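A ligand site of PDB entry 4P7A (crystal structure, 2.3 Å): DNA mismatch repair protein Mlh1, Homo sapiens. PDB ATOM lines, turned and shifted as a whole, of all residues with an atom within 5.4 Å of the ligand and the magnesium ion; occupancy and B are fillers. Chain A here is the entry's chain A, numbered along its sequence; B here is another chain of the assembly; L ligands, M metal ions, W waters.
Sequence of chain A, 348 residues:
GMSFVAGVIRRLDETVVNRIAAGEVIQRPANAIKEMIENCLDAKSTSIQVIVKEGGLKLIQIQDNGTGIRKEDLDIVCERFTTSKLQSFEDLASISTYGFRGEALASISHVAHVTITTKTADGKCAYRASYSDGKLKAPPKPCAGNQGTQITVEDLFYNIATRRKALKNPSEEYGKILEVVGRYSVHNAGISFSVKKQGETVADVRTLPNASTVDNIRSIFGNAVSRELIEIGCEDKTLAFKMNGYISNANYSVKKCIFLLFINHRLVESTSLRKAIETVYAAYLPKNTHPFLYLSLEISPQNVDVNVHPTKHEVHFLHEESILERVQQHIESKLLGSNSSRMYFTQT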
ATOM      1  N   GLU A  35      32.521  10.335 -28.538  1.00  0.00           N
ATOM      2  CA  GLU A  35      31.455   9.339 -28.792  1.00  0.00           C
ATOM      3  C   GLU A  35      31.781   7.975 -28.191  1.00  0.00           C
ATOM      4  O   GLU A  35      30.894   7.261 -27.646  1.00  0.00           O
ATOM      5  CB  GLU A  35      31.240   9.188 -30.319  1.00  0.00           C
ATOM      6  CG  GLU A  35      30.592  10.427 -30.993  1.00  0.00           C
ATOM      7  CD  GLU A  35      29.151  10.676 -30.581  1.00  0.00           C
ATOM      8  OE1 GLU A  35      28.538   9.793 -29.967  1.00  0.00           O
ATOM      9  OE2 GLU A  35      28.593  11.749 -30.866  1.00  0.00           O
ATOM     10  N   MET A  36      33.050   7.574 -28.293  1.00  0.00           N
ATOM     11  CA  MET A  36      33.444   6.249 -27.823  1.00  0.00           C
ATOM     12  C   MET A  36      33.445   6.173 -26.277  1.00  0.00           C
ATOM     13  O   MET A  36      33.012   5.185 -25.709  1.00  0.00           O
ATOM     14  CB  MET A  36      34.806   5.850 -28.401  1.00  0.00           C
ATOM     15  CG  MET A  36      34.687   5.540 -29.899  1.00  0.00           C
ATOM     16  SD  MET A  36      36.166   4.894 -30.715  1.00  0.00           S
ATOM     17  CE  MET A  36      37.034   6.411 -30.653  1.00  0.00           C
ATOM     18  N   ASN A  39      30.011   5.801 -25.031  1.00  0.00           N
ATOM     19  CA  ASN A  39      29.637   4.396 -25.134  1.00  0.00           C
ATOM     20  C   ASN A  39      30.235   3.562 -23.975  1.00  0.00           C
ATOM     21  O   ASN A  39      29.580   2.716 -23.467  1.00  0.00           O
ATOM     22  CB  ASN A  39      30.091   3.828 -26.461  1.00  0.00           C
ATOM     23  CG  ASN A  39      29.290   4.344 -27.628  1.00  0.00           C
ATOM     24  OD1 ASN A  39      28.196   4.822 -27.454  1.00  0.00           O
ATOM     25  ND2 ASN A  39      29.844   4.259 -28.825  1.00  0.00           N
ATOM     26  N   CYS A  40      31.475   3.814 -23.598  1.00  0.00           N
ATOM     27  CA  CYS A  40      32.083   3.132 -22.453  1.00  0.00           C
ATOM     28  C   CYS A  40      31.239   3.385 -21.201  1.00  0.00           C
ATOM     29  O   CYS A  40      30.953   2.453 -20.440  1.00  0.00           O
ATOM     30  CB  CYS A  40      33.472   3.668 -22.208  1.00  0.00           C
ATOM     31  SG  CYS A  40      34.690   3.302 -23.479  1.00  0.00           S
ATOM     32  N   ASP A  42      27.994   4.319 -21.061  1.00  0.00           N
ATOM     33  CA  ASP A  42      26.708   3.661 -21.195  1.00  0.00           C
ATOM     34  C   ASP A  42      26.810   2.141 -20.874  1.00  0.00           C
ATOM     35  O   ASP A  42      25.882   1.541 -20.382  1.00  0.00           O
ATOM     36  CB  ASP A  42      26.135   3.843 -22.581  1.00  0.00           C
ATOM     37  CG  ASP A  42      25.760   5.300 -22.916  1.00  0.00           C
ATOM     38  OD1 ASP A  42      25.477   6.103 -22.040  1.00  0.00           O
ATOM     39  OD2 ASP A  42      25.734   5.620 -24.097  1.00  0.00           O
ATOM     40  N   ALA A  43      27.937   1.538 -21.198  1.00  0.00           N
ATOM     41  CA  ALA A  43      28.163   0.119 -20.972  1.00  0.00           C
ATOM     42  C   ALA A  43      28.749  -0.133 -19.539  1.00  0.00           C
ATOM     43  O   ALA A  43      29.319  -1.156 -19.291  1.00  0.00           O
ATOM     44  CB  ALA A  43      29.093  -0.407 -22.076  1.00  0.00           C
ATOM     45  N   ASP A  64      37.878  -0.507 -22.424  1.00  0.00           N
ATOM     46  CA  ASP A  64      37.054  -0.402 -21.201  1.00  0.00           C
ATOM     47  C   ASP A  64      36.864  -1.776 -20.528  1.00  0.00           C
ATOM     48  O   ASP A  64      37.243  -2.794 -21.102  1.00  0.00           O
ATOM     49  CB  ASP A  64      35.701   0.299 -21.461  1.00  0.00           C
ATOM     50  CG  ASP A  64      34.764  -0.502 -22.387  1.00  0.00           C
ATOM     51  OD1 ASP A  64      34.516  -1.699 -22.093  1.00  0.00           O
ATOM     52  OD2 ASP A  64      34.271   0.080 -23.402  1.00  0.00           O
ATOM     53  N   THR A  67      30.306  -3.791 -20.083  1.00  0.00           N
ATOM     54  CA  THR A  67      29.518  -5.006 -20.307  1.00  0.00           C
ATOM     55  C   THR A  67      29.781  -5.688 -21.623  1.00  0.00           C
ATOM     56  O   THR A  67      29.402  -6.814 -21.806  1.00  0.00           O
ATOM     57  CB  THR A  67      27.992  -4.698 -20.254  1.00  0.00           C
ATOM     58  OG1 THR A  67      27.687  -3.663 -21.182  1.00  0.00           O
ATOM     59  CG2 THR A  67      27.593  -4.249 -18.891  1.00  0.00           C
ATOM     60  N   GLY A  68      30.440  -5.020 -22.553  1.00  0.00           N
ATOM     61  CA  GLY A  68      30.807  -5.654 -23.827  1.00  0.00           C
ATOM     62  C   GLY A  68      29.694  -5.751 -24.841  1.00  0.00           C
ATOM     63  O   GLY A  68      28.556  -5.374 -24.585  1.00  0.00           O
ATOM     64  N   ILE A  69      30.043  -6.256 -26.024  1.00  0.00           N
ATOM     65  CA  ILE A  69      29.093  -6.480 -27.125  1.00  0.00           C
ATOM     66  C   ILE A  69      28.987  -7.992 -27.374  1.00  0.00           C
ATOM     67  O   ILE A  69      29.998  -8.661 -27.585  1.00  0.00           O
ATOM     68  CB  ILE A  69      29.600  -5.794 -28.395  1.00  0.00           C
ATOM     69  CG1 ILE A  69      29.942  -4.325 -28.109  1.00  0.00           C
ATOM     70  CG2 ILE A  69      28.586  -5.944 -29.524  1.00  0.00           C
ATOM     71  CD1 ILE A  69      30.653  -3.555 -29.221  1.00  0.00           C
ATOM     72  N   VAL A  77      26.778  -4.215 -35.460  1.00  0.00           N
ATOM     73  CA  VAL A  77      27.064  -3.144 -34.511  1.00  0.00           C
ATOM     74  C   VAL A  77      27.441  -1.803 -35.171  1.00  0.00           C
ATOM     75  O   VAL A  77      27.006  -0.753 -34.706  1.00  0.00           O
ATOM     76  CB  VAL A  77      28.145  -3.607 -33.453  1.00  0.00           C
ATOM     77  CG1 VAL A  77      29.460  -3.961 -34.126  1.00  0.00           C
ATOM     78  CG2 VAL A  77      28.336  -2.567 -32.357  1.00  0.00           C
ATOM     79  N   THR A  82      21.545   0.844 -35.744  1.00  0.00           N
ATOM     80  CA  THR A  82      21.576  -0.259 -34.816  1.00  0.00           C
ATOM     81  C   THR A  82      22.155   0.171 -33.477  1.00  0.00           C
ATOM     82  O   THR A  82      23.274   0.754 -33.374  1.00  0.00           O
ATOM     83  CB  THR A  82      22.332  -1.474 -35.378  1.00  0.00           C
ATOM     84  OG1 THR A  82      23.731  -1.277 -35.299  1.00  0.00           O
ATOM     85  CG2 THR A  82      21.908  -1.721 -36.832  1.00  0.00           C
ATOM     86  N   THR A  83      21.389  -0.177 -32.438  1.00  0.00           N
ATOM     87  CA  THR A  83      21.608   0.256 -31.092  1.00  0.00           C
ATOM     88  C   THR A  83      20.972  -0.779 -30.096  1.00  0.00           C
ATOM     89  O   THR A  83      19.941  -1.439 -30.400  1.00  0.00           O
ATOM     90  CB  THR A  83      20.898   1.635 -30.880  1.00  0.00           C
ATOM     91  OG1 THR A  83      21.146   2.135 -29.545  1.00  0.00           O
ATOM     92  CG2 THR A  83      19.427   1.471 -31.020  1.00  0.00           C
ATOM     93  N   SER A  84      21.574  -0.872 -28.924  1.00  0.00           N
ATOM     94  CA  SER A  84      20.951  -1.599 -27.821  1.00  0.00           C
ATOM     95  C   SER A  84      20.221  -0.685 -26.825  1.00  0.00           C
ATOM     96  O   SER A  84      19.843  -1.143 -25.771  1.00  0.00           O
ATOM     97  CB  SER A  84      22.021  -2.379 -27.079  1.00  0.00           C
ATOM     98  OG  SER A  84      22.980  -1.500 -26.570  1.00  0.00           O
ATOM     99  N   LYS A  85      20.014   0.577 -27.178  1.00  0.00           N
ATOM    100  CA  LYS A  85      19.449   1.618 -26.300  1.00  0.00           C
ATOM    101  C   LYS A  85      18.030   2.027 -26.745  1.00  0.00           C
ATOM    102  O   LYS A  85      17.642   1.831 -27.905  1.00  0.00           O
ATOM    103  CB  LYS A  85      20.447   2.791 -26.261  1.00  0.00           C
ATOM    104  CG  LYS A  85      21.805   2.344 -25.690  1.00  0.00           C
ATOM    105  CD  LYS A  85      22.973   3.318 -25.845  1.00  0.00           C
ATOM    106  CE  LYS A  85      24.316   2.606 -25.582  1.00  0.00           C
ATOM    107  NZ  LYS A  85      25.548   3.383 -26.075  1.00  0.00           N
ATOM    108  N   PHE A 100      19.758  10.658 -33.857  1.00  0.00           N
ATOM    109  CA  PHE A 100      19.190   9.353 -33.533  1.00  0.00           C
ATOM    110  C   PHE A 100      20.241   8.409 -32.934  1.00  0.00           C
ATOM    111  O   PHE A 100      21.473   8.550 -33.153  1.00  0.00           O
ATOM    112  CB  PHE A 100      18.549   8.709 -34.760  1.00  0.00           C
ATOM    113  CG  PHE A 100      17.373   9.472 -35.286  1.00  0.00           C
ATOM    114  CD1 PHE A 100      16.102   9.270 -34.746  1.00  0.00           C
ATOM    115  CD2 PHE A 100      17.528  10.389 -36.305  1.00  0.00           C
ATOM    116  CE1 PHE A 100      15.030   9.988 -35.203  1.00  0.00           C
ATOM    117  CE2 PHE A 100      16.448  11.100 -36.789  1.00  0.00           C
ATOM    118  CZ  PHE A 100      15.191  10.895 -36.249  1.00  0.00           C
ATOM    119  N   ARG A 101      19.737   7.433 -32.179  1.00  0.00           N
ATOM    120  CA  ARG A 101      20.581   6.401 -31.614  1.00  0.00           C
ATOM    121  C   ARG A 101      21.163   5.659 -32.781  1.00  0.00           C
ATOM    122  O   ARG A 101      20.481   5.480 -33.831  1.00  0.00           O
ATOM    123  CB  ARG A 101      19.765   5.390 -30.753  1.00  0.00           C
ATOM    124  CG  ARG A 101      19.060   5.992 -29.549  1.00  0.00           C
ATOM    125  CD  ARG A 101      19.966   6.081 -28.342  1.00  0.00           C
ATOM    126  NE  ARG A 101      19.205   6.006 -27.103  1.00  0.00           N
ATOM    127  CZ  ARG A 101      19.669   6.396 -25.930  1.00  0.00           C
ATOM    128  NH1 ARG A 101      18.917   6.284 -24.848  1.00  0.00           N
ATOM    129  NH2 ARG A 101      20.859   6.900 -25.856  1.00  0.00           N
ATOM    130  N   GLY A 102      22.370   5.193 -32.591  1.00  0.00           N
ATOM    131  CA  GLY A 102      22.941   4.246 -33.502  1.00  0.00           C
ATOM    132  C   GLY A 102      23.725   4.772 -34.698  1.00  0.00           C
ATOM    133  O   GLY A 102      23.909   4.040 -35.677  1.00  0.00           O
ATOM    134  N   GLU A 103      24.214   6.002 -34.611  1.00  0.00           N
ATOM    135  CA  GLU A 103      24.904   6.635 -35.735  1.00  0.00           C
ATOM    136  C   GLU A 103      26.401   6.789 -35.517  1.00  0.00           C
ATOM    137  O   GLU A 103      27.138   6.936 -36.482  1.00  0.00           O
ATOM    138  CB  GLU A 103      24.373   8.050 -35.919  1.00  0.00           C
ATOM    139  CG  GLU A 103      22.885   8.149 -36.032  1.00  0.00           C
ATOM    140  CD  GLU A 103      22.450   9.144 -37.080  1.00  0.00           C
ATOM    141  OE1 GLU A 103      21.608  10.001 -36.745  1.00  0.00           O
ATOM    142  OE2 GLU A 103      22.984   9.071 -38.203  1.00  0.00           O
ATOM    143  N   ALA A 104      26.851   6.771 -34.272  1.00  0.00           N
ATOM    144  CA  ALA A 104      28.239   7.101 -33.999  1.00  0.00           C
ATOM    145  C   ALA A 104      29.236   6.067 -34.589  1.00  0.00           C
ATOM    146  O   ALA A 104      30.088   6.428 -35.392  1.00  0.00           O
ATOM    147  CB  ALA A 104      28.466   7.308 -32.522  1.00  0.00           C
ATOM    148  N   LEU A 105      29.122   4.795 -34.245  1.00  0.00           N
ATOM    149  CA  LEU A 105      30.091   3.834 -34.788  1.00  0.00           C
ATOM    150  C   LEU A 105      29.915   3.662 -36.289  1.00  0.00           C
ATOM    151  O   LEU A 105      30.902   3.470 -37.016  1.00  0.00           O
ATOM    152  CB  LEU A 105      29.993   2.487 -34.093  1.00  0.00           C
ATOM    153  CG  LEU A 105      30.603   2.482 -32.712  1.00  0.00           C
ATOM    154  CD1 LEU A 105      30.376   1.129 -32.113  1.00  0.00           C
ATOM    155  CD2 LEU A 105      32.085   2.821 -32.770  1.00  0.00           C
ATOM    156  N   ALA A 106      28.686   3.736 -36.778  1.00  0.00           N
ATOM    157  CA  ALA A 106      28.457   3.659 -38.241  1.00  0.00           C
ATOM    158  C   ALA A 106      29.218   4.761 -38.922  1.00  0.00           C
ATOM    159  O   ALA A 106      29.893   4.509 -39.902  1.00  0.00           O
ATOM    160  CB  ALA A 106      27.003   3.802 -38.572  1.00  0.00           C
ATOM    161  N   THR A 149      35.543  -3.989 -23.709  1.00  0.00           N
ATOM    162  CA  THR A 149      35.595  -3.689 -25.133  1.00  0.00           C
ATOM    163  C   THR A 149      36.769  -2.799 -25.397  1.00  0.00           C
ATOM    164  O   THR A 149      37.002  -1.785 -24.655  1.00  0.00           O
ATOM    165  CB  THR A 149      34.285  -2.970 -25.562  1.00  0.00           C
ATOM    166  OG1 THR A 149      33.157  -3.851 -25.335  1.00  0.00           O
ATOM    167  CG2 THR A 149      34.344  -2.609 -27.043  1.00  0.00           C
ATOM    168  N   ILE A 151      38.015  -0.722 -28.740  1.00  0.00           N
ATOM    169  CA  ILE A 151      37.792  -0.251 -30.076  1.00  0.00           C
ATOM    170  C   ILE A 151      39.074   0.419 -30.581  1.00  0.00           C
ATOM    171  O   ILE A 151      39.671   1.240 -29.873  1.00  0.00           O
ATOM    172  CB  ILE A 151      36.707   0.838 -30.201  1.00  0.00           C
ATOM    173  CG1 ILE A 151      35.518   0.599 -29.300  1.00  0.00           C
ATOM    174  CG2 ILE A 151      36.213   0.912 -31.630  1.00  0.00           C
ATOM    175  CD1 ILE A 151      34.413  -0.220 -29.891  1.00  0.00           C
ATOM    176  N   ILE B   9      21.423  -5.710 -29.543  1.00  0.00           N
ATOM    177  CA  ILE B   9      21.371  -4.644 -30.523  1.00  0.00           C
ATOM    178  C   ILE B   9      20.182  -4.922 -31.418  1.00  0.00           C
ATOM    179  O   ILE B   9      20.031  -6.012 -31.904  1.00  0.00           O
ATOM    180  CB  ILE B   9      22.708  -4.592 -31.338  1.00  0.00           C
ATOM    181  CG1 ILE B   9      23.869  -4.167 -30.409  1.00  0.00           C
ATOM    182  CG2 ILE B   9      22.596  -3.616 -32.525  1.00  0.00           C
ATOM    183  CD1 ILE B   9      25.172  -3.890 -31.114  1.00  0.00           C
HETATM  184  P1  LIG L   1      24.272   4.350 -29.622  1.00  0.00           P
HETATM  185  O1  LIG L   1      25.313   4.620 -28.559  1.00  0.00           O
HETATM  186  O2  LIG L   1      23.506   3.055 -29.441  1.00  0.00           O
HETATM  187  O3  LIG L   1      23.411   5.564 -29.906  1.00  0.00           O
HETATM  188  P2  LIG L   1      26.614   3.907 -31.267  1.00  0.00           P
HETATM  189  O4  LIG L   1      27.312   4.907 -30.392  1.00  0.00           O
HETATM  190  O5  LIG L   1      26.889   3.720 -32.717  1.00  0.00           O
HETATM  191  O6  LIG L   1      25.005   4.138 -31.048  1.00  0.00           O
HETATM  192  O7  LIG L   1      26.808   2.431 -30.663  1.00  0.00           O
HETATM  193  C1  LIG L   1      26.111   1.350 -31.238  1.00  0.00           C
HETATM  194  C2  LIG L   1      25.901   0.210 -30.229  1.00  0.00           C
HETATM  195  O8  LIG L   1      27.111  -0.529 -30.152  1.00  0.00           O
HETATM  196  C3  LIG L   1      25.507   0.586 -28.813  1.00  0.00           C
HETATM  197  O9  LIG L   1      24.076   0.665 -28.590  1.00  0.00           O
HETATM  198  C4  LIG L   1      26.090  -0.543 -28.016  1.00  0.00           C
HETATM  199  O10 LIG L   1      25.186  -1.676 -27.900  1.00  0.00           O
HETATM  200  C5  LIG L   1      27.292  -0.961 -28.810  1.00  0.00           C
HETATM  201  N1  LIG L   1      28.533  -0.385 -28.240  1.00  0.00           N
HETATM  202  C6  LIG L   1      29.319   0.569 -28.769  1.00  0.00           C
HETATM  203  N2  LIG L   1      30.365   0.813 -27.977  1.00  0.00           N
HETATM  204  C7  LIG L   1      30.276  -0.023 -26.921  1.00  0.00           C
HETATM  205  C8  LIG L   1      31.081  -0.316 -25.726  1.00  0.00           C
HETATM  206  N3  LIG L   1      32.227   0.373 -25.483  1.00  0.00           N
HETATM  207  N4  LIG L   1      30.668  -1.266 -24.901  1.00  0.00           N
HETATM  208  C9  LIG L   1      29.546  -1.976 -25.136  1.00  0.00           C
HETATM  209  N5  LIG L   1      28.765  -1.770 -26.212  1.00  0.00           N
HETATM  210  C10 LIG L   1      29.099  -0.821 -27.117  1.00  0.00           C
HETATM  211 MG    MG M   1      26.973   5.940 -28.745  1.00  0.00          MG
HETATM  212  O   HOH W   1      25.792   7.198 -29.808  1.00  0.00           O
HETATM  213  O   HOH W   2      26.334   2.760 -35.036  1.00  0.00           O
HETATM  214  O   HOH W   3      27.599   1.609 -25.245  1.00  0.00           O
HETATM  215  O   HOH W   4      28.504   7.296 -28.905  1.00  0.00           O
HETATM  216  O   HOH W   5      26.241  -3.965 -27.198  1.00  0.00           O
HETATM  217  O   HOH W   6      32.270  -2.779 -23.086  1.00  0.00           O
HETATM  218  O   HOH W   7      34.060   2.583 -26.754  1.00  0.00           O
HETATM  219  O   HOH W   8      32.348   2.796 -28.899  1.00  0.00           O
HETATM  220  O   HOH W   9      26.344   6.819 -27.172  1.00  0.00           O
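Water W4 lies within hydrogen-bond range of O of Glu 35 and ND2 of Asn 39.
Water W2 lies within hydrogen-bond range of O5 of the ligand (2.6 Å), O of Gly 102 (2.8 Å) and N of Ala 106 (3.1 Å).
Water W6 lies within hydrogen-bond range of OG1 of Thr 149, OD1 of Asp 64, N4 of the ligand and N of Gly 68.
Water W8 lies within hydrogen-bond range of the side-chain amide nitrogen (ND2) of Asn 39 (2.9 Å) and a nitrogen (N2) of the ligand (3.0 Å).
Water W7 lies within hydrogen-bond range of O of Met 36, N3 of the ligand and SG of Cys 40.
Water W3 bridges NZ of Lys 85 (2.8 Å) and O of Asn 39 (2.9 Å).
Lys 85 touches the magnesium ion.
Of the 25 residues printed, 2 come within 4 Å of the magnesium ion.
The nearest printed residue that does not touch the magnesium ion is Glu 35 (4.3 Å).
Water W9 is bound to the magnesium ion, 1.9 Å away.
An oxygen (O4) of the ligand is bound to the magnesium ion, 2.0 Å away.
Water W1 binds the magnesium ion (2.0 Å).
Water W4 binds the magnesium ion, 2.1 Å away.
The side-chain amide oxygen (OD1) of Asn 39 is bound to the magnesium ion, 2.1 Å away.
O1 of the ligand is bound to the magnesium ion (2.1 Å).
The side-chain hydroxyl (OG1) of Thr 83 is in hydrogen-bond range of an oxygen (O2) of the ligand (2.5 Å).
The backbone NH (N) of Ser 84 lies within hydrogen-bond range of an oxygen (O9) of the ligand (3.0 Å).
An oxygen (O10) of the ligand sits at hydrogen-bond distance from the side-chain hydroxyl (OG) of Ser 84 (2.6 Å).
The side-chain amino group (NZ) of Lys 85 lies within salt-bridge range of an oxygen (O2) of the ligand, at 3.95 Å.
The backbone NH of Gly 102 sits at hydrogen-bond distance from an oxygen (O3) of the ligand, at 2.9 Å.
O5 of the ligand lies within hydrogen-bond range of N of Leu 105 (2.9 Å).
A nitrogen (N3) of the ligand is in hydrogen-bond range of the side-chain carboxylate (OD2) of Asp 64 (2.9 Å).
The backbone NH of Ala 104 is in hydrogen-bond range of an oxygen (O5) of the ligand (3.4 Å).
The side-chain amide oxygen of Asn 39 lies close to the side-chain amino group of Lys 85, at 3.3 Å.
ND2 of Asn 39 sits close to O of Glu 35 (3.4 Å).
The side-chain amino group of Lys 85 lies within salt-bridge range of the side-chain carboxylate of Asp 42 (3.0 Å).
O of Thr 149 is in hydrogen-bond range of N of Asp 64.
The backbone carbonyl oxygen of Val 77 sits at hydrogen-bond distance from the side-chain hydroxyl of Thr 82, 3.4 Å away.
The backbone NH (N) of Thr 67 is in hydrogen-bond range of the backbone carbonyl oxygen (O) of Ala 43, at 2.9 Å.
The side-chain carboxylate (OE1) of Glu 103 sits at hydrogen-bond distance from the backbone NH (N) of Phe 100 (3.5 Å).
O of Met 36 is in hydrogen-bond range of SG of Cys 40.
N of Cys 40 touches N3 of the ligand, at 3.99 Å.
Ala 43 touches the ligand (CB to N4, 3.3 Å).
Gly 68 touches the ligand (O to C9, 3.6 Å).
Ile 69 touches the ligand.
Val 77 touches the ligand.
Thr 82 touches the ligand (O to C1, 3.6 Å).
Arg 101 touches the ligand.
Glu 103 touches the ligand (N to O5, 3.99 Å).
OG1 of Thr 149 touches N4 of the ligand, 3.6 Å away.
Ile 9 of chain B touches the ligand.
Hydrophobic or aromatic side chains within 4 Å of the ligand: Ala 43, Ile 69, Val 77, Ala 104, Leu 105 and Ile 9 of chain B.
Of the 25 residues printed, 18 come within 4 Å of the ligand.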
